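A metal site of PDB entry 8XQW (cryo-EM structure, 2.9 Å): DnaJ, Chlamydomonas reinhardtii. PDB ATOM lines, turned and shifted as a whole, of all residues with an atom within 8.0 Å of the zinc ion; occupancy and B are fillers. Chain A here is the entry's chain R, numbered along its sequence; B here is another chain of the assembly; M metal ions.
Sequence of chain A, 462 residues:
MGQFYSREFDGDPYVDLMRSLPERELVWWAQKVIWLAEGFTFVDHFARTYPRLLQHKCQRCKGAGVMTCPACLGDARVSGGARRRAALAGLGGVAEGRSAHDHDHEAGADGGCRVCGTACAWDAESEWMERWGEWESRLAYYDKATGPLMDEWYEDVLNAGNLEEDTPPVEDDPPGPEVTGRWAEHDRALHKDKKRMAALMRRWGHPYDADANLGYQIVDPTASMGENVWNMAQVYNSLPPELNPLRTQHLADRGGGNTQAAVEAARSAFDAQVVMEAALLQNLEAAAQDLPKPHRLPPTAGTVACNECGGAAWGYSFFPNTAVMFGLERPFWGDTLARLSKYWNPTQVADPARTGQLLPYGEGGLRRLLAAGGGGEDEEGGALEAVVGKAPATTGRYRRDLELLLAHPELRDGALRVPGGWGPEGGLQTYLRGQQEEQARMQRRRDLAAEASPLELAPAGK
N of Cys 69 lies within hydrogen-bond range of O of Gly 302.
O of Ala 301 lies close to SG of Cys 116 (3.4 Å).
The nearest printed residue that does not touch the zinc ion is Ala 301 (5.2 Å).
The zinc ion is bound by SG of Cys 69, SG of Cys 72, SG of Cys 116 and SG of Cys 113.
The zinc ion has four donor atoms within binding distance.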
ATOM      1  N   THR A  68     -35.138  11.212 -14.729  1.00  0.00           N
ATOM      2  CA  THR A  68     -34.652  10.003 -14.096  1.00  0.00           C
ATOM      3  C   THR A  68     -33.225   9.703 -14.508  1.00  0.00           C
ATOM      4  O   THR A  68     -32.765  10.134 -15.564  1.00  0.00           O
ATOM      5  CB  THR A  68     -35.536   8.812 -14.456  1.00  0.00           C
ATOM      6  OG1 THR A  68     -36.903   9.236 -14.504  1.00  0.00           O
ATOM      7  CG2 THR A  68     -35.404   7.720 -13.433  1.00  0.00           C
ATOM      8  N   CYS A  69     -32.519   8.961 -13.668  1.00  0.00           N
ATOM      9  CA  CYS A  69     -31.242   8.357 -14.026  1.00  0.00           C
ATOM     10  C   CYS A  69     -31.483   6.896 -14.356  1.00  0.00           C
ATOM     11  O   CYS A  69     -31.630   6.084 -13.437  1.00  0.00           O
ATOM     12  CB  CYS A  69     -30.228   8.489 -12.903  1.00  0.00           C
ATOM     13  SG  CYS A  69     -28.743   7.521 -13.165  1.00  0.00           S
ATOM     14  N   PRO A  70     -31.534   6.507 -15.638  1.00  0.00           N
ATOM     15  CA  PRO A  70     -32.059   5.173 -15.976  1.00  0.00           C
ATOM     16  C   PRO A  70     -31.226   4.021 -15.440  1.00  0.00           C
ATOM     17  O   PRO A  70     -31.788   2.976 -15.116  1.00  0.00           O
ATOM     18  CB  PRO A  70     -32.082   5.179 -17.507  1.00  0.00           C
ATOM     19  CG  PRO A  70     -31.982   6.611 -17.896  1.00  0.00           C
ATOM     20  CD  PRO A  70     -31.159   7.254 -16.846  1.00  0.00           C
ATOM     21  N   ALA A  71     -29.901   4.187 -15.336  1.00  0.00           N
ATOM     22  CA  ALA A  71     -29.050   3.126 -14.836  1.00  0.00           C
ATOM     23  C   ALA A  71     -29.492   2.618 -13.475  1.00  0.00           C
ATOM     24  O   ALA A  71     -29.331   1.433 -13.179  1.00  0.00           O
ATOM     25  CB  ALA A  71     -27.604   3.605 -14.753  1.00  0.00           C
ATOM     26  N   CYS A  72     -30.070   3.489 -12.643  1.00  0.00           N
ATOM     27  CA  CYS A  72     -30.521   3.119 -11.314  1.00  0.00           C
ATOM     28  C   CYS A  72     -31.951   2.581 -11.305  1.00  0.00           C
ATOM     29  O   CYS A  72     -32.621   2.632 -10.276  1.00  0.00           O
ATOM     30  CB  CYS A  72     -30.423   4.325 -10.376  1.00  0.00           C
ATOM     31  SG  CYS A  72     -28.874   5.235 -10.515  1.00  0.00           S
ATOM     32  N   LEU A  73     -32.428   2.056 -12.441  1.00  0.00           N
ATOM     33  CA  LEU A  73     -33.753   1.445 -12.510  1.00  0.00           C
ATOM     34  C   LEU A  73     -33.725  -0.060 -12.342  1.00  0.00           C
ATOM     35  O   LEU A  73     -34.621  -0.605 -11.682  1.00  0.00           O
ATOM     36  CB  LEU A  73     -34.428   1.795 -13.836  1.00  0.00           C
ATOM     37  CG  LEU A  73     -35.485   2.909 -13.811  1.00  0.00           C
ATOM     38  CD1 LEU A  73     -36.282   2.888 -15.084  1.00  0.00           C
ATOM     39  CD2 LEU A  73     -36.381   2.736 -12.630  1.00  0.00           C
ATOM     40  N   GLY A 112     -21.840   3.812  -5.672  1.00  0.00           N
ATOM     41  CA  GLY A 112     -23.107   3.949  -6.366  1.00  0.00           C
ATOM     42  C   GLY A 112     -23.005   4.911  -7.536  1.00  0.00           C
ATOM     43  O   GLY A 112     -21.909   5.223  -8.011  1.00  0.00           O
ATOM     44  N   CYS A 113     -24.161   5.375  -8.005  1.00  0.00           N
ATOM     45  CA  CYS A 113     -24.170   6.360  -9.075  1.00  0.00           C
ATOM     46  C   CYS A 113     -23.650   7.685  -8.534  1.00  0.00           C
ATOM     47  O   CYS A 113     -24.076   8.146  -7.475  1.00  0.00           O
ATOM     48  CB  CYS A 113     -25.577   6.519  -9.633  1.00  0.00           C
ATOM     49  SG  CYS A 113     -25.669   7.086 -11.345  1.00  0.00           S
ATOM     50  N   ARG A 114     -22.711   8.280  -9.255  1.00  0.00           N
ATOM     51  CA  ARG A 114     -22.113   9.550  -8.871  1.00  0.00           C
ATOM     52  C   ARG A 114     -22.802  10.733  -9.520  1.00  0.00           C
ATOM     53  O   ARG A 114     -22.475  11.870  -9.203  1.00  0.00           O
ATOM     54  CB  ARG A 114     -20.629   9.560  -9.230  1.00  0.00           C
ATOM     55  CG  ARG A 114     -19.750   8.864  -8.221  1.00  0.00           C
ATOM     56  CD  ARG A 114     -19.936   9.458  -6.848  1.00  0.00           C
ATOM     57  NE  ARG A 114     -18.734   9.363  -6.045  1.00  0.00           N
ATOM     58  CZ  ARG A 114     -18.319   8.262  -5.444  1.00  0.00           C
ATOM     59  NH1 ARG A 114     -19.022   7.136  -5.564  1.00  0.00           N
ATOM     60  NH2 ARG A 114     -17.207   8.264  -4.740  1.00  0.00           N
ATOM     61  N   VAL A 115     -23.745  10.484 -10.421  1.00  0.00           N
ATOM     62  CA  VAL A 115     -24.374  11.542 -11.185  1.00  0.00           C
ATOM     63  C   VAL A 115     -25.698  12.002 -10.582  1.00  0.00           C
ATOM     64  O   VAL A 115     -26.118  13.127 -10.853  1.00  0.00           O
ATOM     65  CB  VAL A 115     -24.577  11.089 -12.644  1.00  0.00           C
ATOM     66  CG1 VAL A 115     -24.688  12.278 -13.549  1.00  0.00           C
ATOM     67  CG2 VAL A 115     -23.441  10.200 -13.065  1.00  0.00           C
ATOM     68  N   CYS A 116     -26.352  11.176  -9.780  1.00  0.00           N
ATOM     69  CA  CYS A 116     -27.756  11.378  -9.460  1.00  0.00           C
ATOM     70  C   CYS A 116     -27.922  11.672  -7.977  1.00  0.00           C
ATOM     71  O   CYS A 116     -27.914  10.763  -7.153  1.00  0.00           O
ATOM     72  CB  CYS A 116     -28.579  10.159  -9.887  1.00  0.00           C
ATOM     73  SG  CYS A 116     -28.253   8.599  -9.065  1.00  0.00           S
ATOM     74  N   GLY A 117     -28.069  12.958  -7.643  1.00  0.00           N
ATOM     75  CA  GLY A 117     -28.586  13.377  -6.359  1.00  0.00           C
ATOM     76  C   GLY A 117     -27.864  12.850  -5.144  1.00  0.00           C
ATOM     77  O   GLY A 117     -26.857  12.137  -5.251  1.00  0.00           O
ATOM     78  N   THR A 300     -32.917  14.226  -5.813  1.00  0.00           N
ATOM     79  CA  THR A 300     -32.665  13.213  -4.802  1.00  0.00           C
ATOM     80  C   THR A 300     -31.974  12.007  -5.424  1.00  0.00           C
ATOM     81  O   THR A 300     -31.536  12.037  -6.576  1.00  0.00           O
ATOM     82  CB  THR A 300     -33.969  12.829  -4.123  1.00  0.00           C
ATOM     83  OG1 THR A 300     -35.022  12.819  -5.084  1.00  0.00           O
ATOM     84  CG2 THR A 300     -34.298  13.818  -3.035  1.00  0.00           C
ATOM     85  N   ALA A 301     -31.864  10.935  -4.660  1.00  0.00           N
ATOM     86  CA  ALA A 301     -30.920   9.866  -4.942  1.00  0.00           C
ATOM     87  C   ALA A 301     -31.240   9.070  -6.187  1.00  0.00           C
ATOM     88  O   ALA A 301     -30.460   8.174  -6.517  1.00  0.00           O
ATOM     89  CB  ALA A 301     -30.839   8.916  -3.755  1.00  0.00           C
ATOM     90  N   GLY A 302     -32.320   9.338  -6.899  1.00  0.00           N
ATOM     91  CA  GLY A 302     -32.581   8.529  -8.068  1.00  0.00           C
ATOM     92  C   GLY A 302     -32.799   9.359  -9.317  1.00  0.00           C
ATOM     93  O   GLY A 302     -33.093   8.811 -10.374  1.00  0.00           O
ATOM     94  N   THR A 303     -32.658  10.668  -9.192  1.00  0.00           N
ATOM     95  CA  THR A 303     -33.050  11.582 -10.246  1.00  0.00           C
ATOM     96  C   THR A 303     -31.954  12.613 -10.472  1.00  0.00           C
ATOM     97  O   THR A 303     -31.188  12.946  -9.574  1.00  0.00           O
ATOM     98  CB  THR A 303     -34.331  12.318  -9.888  1.00  0.00           C
ATOM     99  OG1 THR A 303     -34.036  13.316  -8.911  1.00  0.00           O
ATOM    100  CG2 THR A 303     -35.345  11.388  -9.317  1.00  0.00           C
ATOM    101  N   VAL A 304     -31.902  13.123 -11.694  1.00  0.00           N
ATOM    102  CA  VAL A 304     -30.978  14.181 -12.071  1.00  0.00           C
ATOM    103  C   VAL A 304     -31.797  15.391 -12.467  1.00  0.00           C
ATOM    104  O   VAL A 304     -33.011  15.306 -12.646  1.00  0.00           O
ATOM    105  CB  VAL A 304     -30.035  13.766 -13.200  1.00  0.00           C
ATOM    106  CG1 VAL A 304     -29.574  12.346 -12.984  1.00  0.00           C
ATOM    107  CG2 VAL A 304     -30.724  13.869 -14.520  1.00  0.00           C
ATOM    108  N   ALA B 209     -35.037   6.826  -5.369  1.00  0.00           N
ATOM    109  CA  ALA B 209     -34.470   5.486  -5.336  1.00  0.00           C
ATOM    110  C   ALA B 209     -34.978   4.695  -4.139  1.00  0.00           C
ATOM    111  O   ALA B 209     -35.262   3.506  -4.255  1.00  0.00           O
ATOM    112  CB  ALA B 209     -32.956   5.571  -5.323  1.00  0.00           C
HETATM  113 ZN    ZN M   1     -28.048   7.342 -11.036  1.00  0.00          ZN
